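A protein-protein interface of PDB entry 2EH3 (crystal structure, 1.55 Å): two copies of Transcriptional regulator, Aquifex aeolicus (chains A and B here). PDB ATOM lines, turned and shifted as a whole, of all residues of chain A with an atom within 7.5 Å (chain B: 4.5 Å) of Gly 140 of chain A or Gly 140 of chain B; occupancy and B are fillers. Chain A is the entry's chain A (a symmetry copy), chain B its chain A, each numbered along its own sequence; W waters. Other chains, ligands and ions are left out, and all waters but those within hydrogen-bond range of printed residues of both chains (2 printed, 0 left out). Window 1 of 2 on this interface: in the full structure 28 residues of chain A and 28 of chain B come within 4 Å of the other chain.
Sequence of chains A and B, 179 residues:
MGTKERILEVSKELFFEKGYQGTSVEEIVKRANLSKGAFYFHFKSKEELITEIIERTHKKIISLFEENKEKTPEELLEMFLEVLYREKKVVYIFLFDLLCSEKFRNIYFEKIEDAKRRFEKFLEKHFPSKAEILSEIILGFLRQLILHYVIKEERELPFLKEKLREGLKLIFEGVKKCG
The side-chain amide oxygen (OE1) of Gln 144 of chain B is in hydrogen-bond range of the guanidinium group (NH1) of Arg 143 of chain A, at 2.7 Å. The guanidinium group (NH1) of Arg 143 of chain B lies within hydrogen-bond range of the side-chain amide oxygen (OE1) of Gln 144 of chain A (2.7 Å).
Glu 136 of chain A touches Phe 141 of chain B (CB to CE1, 3.7 Å). Glu 136 of chain A touches Gln 144 of chain B (OE1 to CG, 3.5 Å). Ile 137 of chain B touches Ile 137 of chain A (CG2 to CG2, 3.7 Å). Leu 139 of chain A touches Gln 144 of chain B (C to OE1, 3.7 Å). N of Gly 140 of chain A touches OE1 of Gln 144 of chain B (3.5 Å). CE1 of Phe 141 of chain A touches CB of Glu 136 of chain B, 3.7 Å away. Glu 136 of chain B touches Gln 144 of chain A (OE1 to CG, 3.5 Å). C of Leu 139 of chain B touches OE1 of Gln 144 of chain A, 3.7 Å away. Gly 140 of chain B touches Gln 144 of chain A. OE1 of Glu 136 of chain B touches CD2 of Leu 145 of chain A (3.96 Å).
Ser 135 of chain A touches none of the printed residues of chain B. Of the printed residues of chain B, Leu 139 of chain A touches Gln 144. Of chain B, only Gly 140 and Gln 144 come within 4 Å of Gly 140 of chain A. Ile 146 of chain A touches none of the printed residues of chain B. Of the printed residues of chain A, Phe 141 of chain B touches Glu 136 (3.7 Å) and Ile 137 (3.7 Å). The nearest residue of chain A that does not touch Gly 140 of chain B is Phe 141 of chain A (4.1 Å). The nearest printed residue of chain B that does not touch Leu 139 of chain A is Gly 140 of chain B (5.6 Å).
Printed residues of chain B that touch a printed residue of chain A: Glu 136, Ile 137, Leu 139, Gly 140, Phe 141, Arg 143 and Gln 144. Hydrophobic or aromatic side chains of chain B within 4 Å of the printed part of chain A: Ile 137, Leu 139 and Phe 141. Hydrophobic or aromatic side chains of chain A within 4 Å of the printed part of chain B: Ile 137, Leu 139, Phe 141 and Leu 145. Along chain A the printed residues that touch a printed residue of chain B span positions 136 to 145. Among the printed residues, 15 pairs touch across the chains. Among the printed residues, no Asp or Glu carboxylate lies within 4 Å of a Lys or Arg side-chain nitrogen of the other chain.
Glu 136 of chain A touches Gln 144 of chain B, and with the chains exchanged Gln 144 of chain A touches Glu 136 of chain B. Ile 137 of chain A touches its own counterpart, Ile 137 of chain B. Ile 137 of chain A touches Phe 141 of chain B, and with the chains exchanged Phe 141 of chain A touches Ile 137 of chain B. Arg 143 of chain A touches Gln 144 of chain B, and with the chains exchanged Gln 144 of chain A touches Arg 143 of chain B. Positions printed for both chains: 136, 137, 138, 139, 140, 141, 142, 143 and 144.
Water W2 lies within hydrogen-bond range of the side-chain carboxylate of Glu 136 of chain A (2.5 Å) and the side-chain amide nitrogen of Gln 144 of chain B (3.0 Å). Water W1 lies within hydrogen-bond range of OE1 of Glu 136 of chain B and NE2 of Gln 144 of chain A.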
ATOM      1  N   PHE A 119      -8.662  17.274  -4.230  1.00  0.00           N
ATOM      2  CA  PHE A 119      -8.099  16.340  -3.304  1.00  0.00           C
ATOM      3  C   PHE A 119      -6.956  15.579  -3.989  1.00  0.00           C
ATOM      4  O   PHE A 119      -5.893  15.337  -3.396  1.00  0.00           O
ATOM      5  CB  PHE A 119      -9.201  15.393  -2.828  1.00  0.00           C
ATOM      6  CG  PHE A 119      -8.767  14.458  -1.756  1.00  0.00           C
ATOM      7  CD1 PHE A 119      -7.882  14.857  -0.754  1.00  0.00           C
ATOM      8  CD2 PHE A 119      -9.275  13.154  -1.741  1.00  0.00           C
ATOM      9  CE1 PHE A 119      -7.506  13.972   0.256  1.00  0.00           C
ATOM     10  CE2 PHE A 119      -8.910  12.269  -0.745  1.00  0.00           C
ATOM     11  CZ  PHE A 119      -8.027  12.672   0.256  1.00  0.00           C
ATOM     12  N   LEU A 134      -6.211   6.684  -3.974  1.00  0.00           N
ATOM     13  CA  LEU A 134      -6.549   7.167  -2.639  1.00  0.00           C
ATOM     14  C   LEU A 134      -7.718   8.124  -2.672  1.00  0.00           C
ATOM     15  O   LEU A 134      -8.550   8.127  -1.753  1.00  0.00           O
ATOM     16  CB  LEU A 134      -5.346   7.887  -2.030  1.00  0.00           C
ATOM     17  CG  LEU A 134      -4.193   7.015  -1.543  1.00  0.00           C
ATOM     18  CD1 LEU A 134      -2.926   7.886  -1.307  1.00  0.00           C
ATOM     19  CD2 LEU A 134      -4.641   6.301  -0.265  1.00  0.00           C
ATOM     20  N   SER A 135      -7.817   8.939  -3.720  1.00  0.00           N
ATOM     21  CA  SER A 135      -8.922   9.888  -3.756  1.00  0.00           C
ATOM     22  C   SER A 135     -10.261   9.158  -3.831  1.00  0.00           C
ATOM     23  O   SER A 135     -11.211   9.589  -3.179  1.00  0.00           O
ATOM     24  CB  SER A 135      -8.788  10.867  -4.937  1.00  0.00           C
ATOM     25  OG  SER A 135      -9.024  10.220  -6.185  1.00  0.00           O
ATOM     26  N   GLU A 136     -10.329   8.065  -4.606  1.00  0.00           N
ATOM     27  CA  GLU A 136     -11.535   7.265  -4.760  1.00  0.00           C
ATOM     28  C   GLU A 136     -11.891   6.598  -3.438  1.00  0.00           C
ATOM     29  O   GLU A 136     -13.056   6.637  -2.978  1.00  0.00           O
ATOM     30  CB  GLU A 136     -11.321   6.163  -5.797  1.00  0.00           C
ATOM     31  CG  GLU A 136     -10.927   6.652  -7.194  1.00  0.00           C
ATOM     32  CD  GLU A 136     -12.105   7.028  -8.063  1.00  0.00           C
ATOM     33  OE1 GLU A 136     -13.258   7.065  -7.553  1.00  0.00           O
ATOM     34  OE2 GLU A 136     -11.865   7.308  -9.251  1.00  0.00           O
ATOM     35  N   ILE A 137     -10.889   5.972  -2.830  1.00  0.00           N
ATOM     36  CA  ILE A 137     -11.098   5.289  -1.557  1.00  0.00           C
ATOM     37  C   ILE A 137     -11.574   6.246  -0.464  1.00  0.00           C
ATOM     38  O   ILE A 137     -12.580   6.005   0.220  1.00  0.00           O
ATOM     39  CB  ILE A 137      -9.800   4.654  -1.040  1.00  0.00           C
ATOM     40  CG1 ILE A 137      -9.342   3.515  -1.976  1.00  0.00           C
ATOM     41  CG2 ILE A 137     -10.033   4.129   0.379  1.00  0.00           C
ATOM     42  CD1 ILE A 137      -7.907   3.042  -1.713  1.00  0.00           C
ATOM     43  N   ILE A 138     -10.835   7.329  -0.291  1.00  0.00           N
ATOM     44  CA  ILE A 138     -11.146   8.258   0.779  1.00  0.00           C
ATOM     45  C   ILE A 138     -12.440   9.012   0.569  1.00  0.00           C
ATOM     46  O   ILE A 138     -13.219   9.167   1.515  1.00  0.00           O
ATOM     47  CB  ILE A 138      -9.952   9.189   1.002  1.00  0.00           C
ATOM     48  CG1 ILE A 138      -8.774   8.332   1.487  1.00  0.00           C
ATOM     49  CG2 ILE A 138     -10.290  10.255   2.052  1.00  0.00           C
ATOM     50  CD1 ILE A 138      -7.447   9.078   1.563  1.00  0.00           C
ATOM     51  N   LEU A 139     -12.717   9.471  -0.646  1.00  0.00           N
ATOM     52  CA  LEU A 139     -13.995  10.143  -0.858  1.00  0.00           C
ATOM     53  C   LEU A 139     -15.136   9.152  -0.653  1.00  0.00           C
ATOM     54  O   LEU A 139     -16.175   9.507  -0.106  1.00  0.00           O
ATOM     55  CB  LEU A 139     -14.092  10.739  -2.265  1.00  0.00           C
ATOM     56  CG  LEU A 139     -13.288  12.015  -2.499  1.00  0.00           C
ATOM     57  CD1 LEU A 139     -13.582  12.541  -3.913  1.00  0.00           C
ATOM     58  CD2 LEU A 139     -13.670  13.067  -1.482  1.00  0.00           C
ATOM     59  N   GLY A 140     -14.937   7.911  -1.089  1.00  0.00           N
ATOM     60  CA  GLY A 140     -15.961   6.895  -0.903  1.00  0.00           C
ATOM     61  C   GLY A 140     -16.226   6.649   0.574  1.00  0.00           C
ATOM     62  O   GLY A 140     -17.378   6.602   1.020  1.00  0.00           O
ATOM     63  N   PHE A 141     -15.151   6.538   1.336  1.00  0.00           N
ATOM     64  CA  PHE A 141     -15.247   6.301   2.776  1.00  0.00           C
ATOM     65  C   PHE A 141     -15.929   7.477   3.477  1.00  0.00           C
ATOM     66  O   PHE A 141     -16.814   7.276   4.311  1.00  0.00           O
ATOM     67  CB  PHE A 141     -13.815   6.053   3.290  1.00  0.00           C
ATOM     68  CG  PHE A 141     -13.675   5.947   4.794  1.00  0.00           C
ATOM     69  CD1 PHE A 141     -14.553   5.178   5.563  1.00  0.00           C
ATOM     70  CD2 PHE A 141     -12.598   6.579   5.429  1.00  0.00           C
ATOM     71  CE1 PHE A 141     -14.349   5.036   6.959  1.00  0.00           C
ATOM     72  CE2 PHE A 141     -12.394   6.433   6.798  1.00  0.00           C
ATOM     73  CZ  PHE A 141     -13.272   5.656   7.559  1.00  0.00           C
ATOM     74  N   LEU A 142     -15.541   8.697   3.126  1.00  0.00           N
ATOM     75  CA  LEU A 142     -16.139   9.877   3.759  1.00  0.00           C
ATOM     76  C   LEU A 142     -17.625   9.909   3.430  1.00  0.00           C
ATOM     77  O   LEU A 142     -18.455  10.173   4.308  1.00  0.00           O
ATOM     78  CB  LEU A 142     -15.432  11.129   3.261  1.00  0.00           C
ATOM     79  CG  LEU A 142     -15.844  12.484   3.811  1.00  0.00           C
ATOM     80  CD1 LEU A 142     -15.651  12.515   5.323  1.00  0.00           C
ATOM     81  CD2 LEU A 142     -14.991  13.544   3.118  1.00  0.00           C
ATOM     82  N   ARG A 143     -17.986   9.619   2.180  1.00  0.00           N
ATOM     83  CA  ARG A 143     -19.401   9.624   1.804  1.00  0.00           C
ATOM     84  C   ARG A 143     -20.189   8.531   2.564  1.00  0.00           C
ATOM     85  O   ARG A 143     -21.302   8.781   3.032  1.00  0.00           O
ATOM     86  CB  ARG A 143     -19.500   9.529   0.280  1.00  0.00           C
ATOM     87  CG  ARG A 143     -18.865  10.810  -0.323  1.00  0.00           C
ATOM     88  CD  ARG A 143     -18.635  10.746  -1.828  1.00  0.00           C
ATOM     89  NE  ARG A 143     -19.878  10.843  -2.588  1.00  0.00           N
ATOM     90  CZ  ARG A 143     -19.951  10.680  -3.906  1.00  0.00           C
ATOM     91  NH1 ARG A 143     -18.866  10.408  -4.596  1.00  0.00           N
ATOM     92  NH2 ARG A 143     -21.105  10.814  -4.536  1.00  0.00           N
ATOM     93  N   GLN A 144     -19.588   7.349   2.756  1.00  0.00           N
ATOM     94  CA  GLN A 144     -20.214   6.254   3.503  1.00  0.00           C
ATOM     95  C   GLN A 144     -20.500   6.742   4.936  1.00  0.00           C
ATOM     96  O   GLN A 144     -21.594   6.540   5.476  1.00  0.00           O
ATOM     97  CB  GLN A 144     -19.273   5.035   3.551  1.00  0.00           C
ATOM     98  CG  GLN A 144     -19.674   3.880   4.485  1.00  0.00           C
ATOM     99  CD  GLN A 144     -20.621   2.869   3.853  1.00  0.00           C
ATOM    100  OE1 GLN A 144     -20.779   2.822   2.635  1.00  0.00           O
ATOM    101  NE2 GLN A 144     -21.234   2.036   4.683  1.00  0.00           N
ATOM    102  N   LEU A 145     -19.521   7.404   5.548  1.00  0.00           N
ATOM    103  CA  LEU A 145     -19.733   7.887   6.916  1.00  0.00           C
ATOM    104  C   LEU A 145     -20.809   8.950   6.997  1.00  0.00           C
ATOM    105  O   LEU A 145     -21.604   8.964   7.944  1.00  0.00           O
ATOM    106  CB  LEU A 145     -18.444   8.454   7.510  1.00  0.00           C
ATOM    107  CG  LEU A 145     -17.251   7.513   7.659  1.00  0.00           C
ATOM    108  CD1 LEU A 145     -16.091   8.357   8.218  1.00  0.00           C
ATOM    109  CD2 LEU A 145     -17.584   6.339   8.565  1.00  0.00           C
ATOM    110  N   ILE A 146     -20.859   9.852   6.031  1.00  0.00           N
ATOM    111  CA  ILE A 146     -21.874  10.895   6.097  1.00  0.00           C
ATOM    112  C   ILE A 146     -23.253  10.320   5.856  1.00  0.00           C
ATOM    113  O   ILE A 146     -24.216  10.677   6.532  1.00  0.00           O
ATOM    114  CB  ILE A 146     -21.600  11.991   5.049  1.00  0.00           C
ATOM    115  CG1 ILE A 146     -20.288  12.702   5.381  1.00  0.00           C
ATOM    116  CG2 ILE A 146     -22.777  12.993   5.001  1.00  0.00           C
ATOM    117  CD1 ILE A 146     -20.267  13.382   6.720  1.00  0.00           C
ATOM    118  N   GLU B 136     -16.380  -0.225   6.414  1.00  0.00           N
ATOM    119  CA  GLU B 136     -16.780   1.142   6.113  1.00  0.00           C
ATOM    120  C   GLU B 136     -16.001   1.660   4.910  1.00  0.00           C
ATOM    121  O   GLU B 136     -16.576   2.235   3.957  1.00  0.00           O
ATOM    122  CB  GLU B 136     -16.482   2.063   7.295  1.00  0.00           C
ATOM    123  CG  GLU B 136     -17.166   1.677   8.609  1.00  0.00           C
ATOM    124  CD  GLU B 136     -18.573   2.212   8.744  1.00  0.00           C
ATOM    125  OE1 GLU B 136     -19.115   2.774   7.754  1.00  0.00           O
ATOM    126  OE2 GLU B 136     -19.138   2.047   9.840  1.00  0.00           O
ATOM    127  N   ILE B 137     -14.687   1.469   4.959  1.00  0.00           N
ATOM    128  CA  ILE B 137     -13.826   1.922   3.871  1.00  0.00           C
ATOM    129  C   ILE B 137     -14.186   1.260   2.541  1.00  0.00           C
ATOM    130  O   ILE B 137     -14.386   1.926   1.515  1.00  0.00           O
ATOM    131  CB  ILE B 137     -12.354   1.580   4.141  1.00  0.00           C
ATOM    132  CG1 ILE B 137     -11.826   2.372   5.357  1.00  0.00           C
ATOM    133  CG2 ILE B 137     -11.533   1.897   2.889  1.00  0.00           C
ATOM    134  CD1 ILE B 137     -10.479   1.863   5.882  1.00  0.00           C
ATOM    135  N   ILE B 138     -14.250  -0.060   2.560  1.00  0.00           N
ATOM    136  CA  ILE B 138     -14.495  -0.794   1.332  1.00  0.00           C
ATOM    137  C   ILE B 138     -15.889  -0.600   0.779  1.00  0.00           C
ATOM    138  O   ILE B 138     -16.049  -0.424  -0.433  1.00  0.00           O
ATOM    139  CB  ILE B 138     -14.148  -2.268   1.546  1.00  0.00           C
ATOM    140  CG1 ILE B 138     -12.640  -2.358   1.823  1.00  0.00           C
ATOM    141  CG2 ILE B 138     -14.500  -3.091   0.301  1.00  0.00           C
ATOM    142  CD1 ILE B 138     -12.165  -3.740   2.259  1.00  0.00           C
ATOM    143  N   LEU B 139     -16.913  -0.600   1.626  1.00  0.00           N
ATOM    144  CA  LEU B 139     -18.250  -0.350   1.096  1.00  0.00           C
ATOM    145  C   LEU B 139     -18.326   1.070   0.545  1.00  0.00           C
ATOM    146  O   LEU B 139     -18.962   1.306  -0.478  1.00  0.00           O
ATOM    147  CB  LEU B 139     -19.326  -0.532   2.169  1.00  0.00           C
ATOM    148  CG  LEU B 139     -19.652  -1.977   2.539  1.00  0.00           C
ATOM    149  CD1 LEU B 139     -20.820  -1.988   3.538  1.00  0.00           C
ATOM    150  CD2 LEU B 139     -20.041  -2.757   1.303  1.00  0.00           C
ATOM    151  N   GLY B 140     -17.674   2.011   1.223  1.00  0.00           N
ATOM    152  CA  GLY B 140     -17.668   3.386   0.748  1.00  0.00           C
ATOM    153  C   GLY B 140     -17.002   3.491  -0.616  1.00  0.00           C
ATOM    154  O   GLY B 140     -17.525   4.128  -1.537  1.00  0.00           O
ATOM    155  N   PHE B 141     -15.869   2.823  -0.751  1.00  0.00           N
ATOM    156  CA  PHE B 141     -15.115   2.828  -2.005  1.00  0.00           C
ATOM    157  C   PHE B 141     -15.924   2.178  -3.128  1.00  0.00           C
ATOM    158  O   PHE B 141     -15.997   2.717  -4.235  1.00  0.00           O
ATOM    159  CB  PHE B 141     -13.783   2.101  -1.734  1.00  0.00           C
ATOM    160  CG  PHE B 141     -12.920   1.854  -2.953  1.00  0.00           C
ATOM    161  CD1 PHE B 141     -12.688   2.850  -3.906  1.00  0.00           C
ATOM    162  CD2 PHE B 141     -12.280   0.616  -3.102  1.00  0.00           C
ATOM    163  CE1 PHE B 141     -11.812   2.611  -4.995  1.00  0.00           C
ATOM    164  CE2 PHE B 141     -11.416   0.385  -4.167  1.00  0.00           C
ATOM    165  CZ  PHE B 141     -11.182   1.389  -5.111  1.00  0.00           C
ATOM    166  N   LEU B 142     -16.547   1.041  -2.845  1.00  0.00           N
ATOM    167  CA  LEU B 142     -17.334   0.349  -3.871  1.00  0.00           C
ATOM    168  C   LEU B 142     -18.489   1.249  -4.291  1.00  0.00           C
ATOM    169  O   LEU B 142     -18.778   1.379  -5.487  1.00  0.00           O
ATOM    170  CB  LEU B 142     -17.835  -0.976  -3.314  1.00  0.00           C
ATOM    171  CG  LEU B 142     -18.641  -1.901  -4.210  1.00  0.00           C
ATOM    172  CD1 LEU B 142     -17.820  -2.290  -5.434  1.00  0.00           C
ATOM    173  CD2 LEU B 142     -19.026  -3.126  -3.384  1.00  0.00           C
ATOM    174  N   ARG B 143     -19.146   1.897  -3.329  1.00  0.00           N
ATOM    175  CA  ARG B 143     -20.259   2.784  -3.671  1.00  0.00           C
ATOM    176  C   ARG B 143     -19.781   3.987  -4.519  1.00  0.00           C
ATOM    177  O   ARG B 143     -20.443   4.362  -5.490  1.00  0.00           O
ATOM    178  CB  ARG B 143     -20.987   3.171  -2.382  1.00  0.00           C
ATOM    179  CG  ARG B 143     -21.602   1.883  -1.773  1.00  0.00           C
ATOM    180  CD  ARG B 143     -22.122   2.049  -0.350  1.00  0.00           C
ATOM    181  NE  ARG B 143     -23.357   2.826  -0.293  1.00  0.00           N
ATOM    182  CZ  ARG B 143     -23.930   3.217   0.841  1.00  0.00           C
ATOM    183  NH1 ARG B 143     -23.380   2.912   1.996  1.00  0.00           N
ATOM    184  NH2 ARG B 143     -25.067   3.891   0.821  1.00  0.00           N
ATOM    185  N   GLN B 144     -18.603   4.541  -4.206  1.00  0.00           N
ATOM    186  CA  GLN B 144     -18.023   5.653  -4.966  1.00  0.00           C
ATOM    187  C   GLN B 144     -17.822   5.195  -6.424  1.00  0.00           C
ATOM    188  O   GLN B 144     -18.172   5.905  -7.373  1.00  0.00           O
ATOM    189  CB  GLN B 144     -16.665   6.061  -4.362  1.00  0.00           C
ATOM    190  CG  GLN B 144     -15.814   7.057  -5.168  1.00  0.00           C
ATOM    191  CD  GLN B 144     -16.145   8.519  -4.899  1.00  0.00           C
ATOM    192  OE1 GLN B 144     -16.795   8.851  -3.910  1.00  0.00           O
ATOM    193  NE2 GLN B 144     -15.671   9.400  -5.768  1.00  0.00           N
HETATM  194  O   HOH W   1     -21.624   2.510   7.660  1.00  0.00           O
HETATM  195  O   HOH W   2     -14.804   8.758  -8.610  1.00  0.00           O
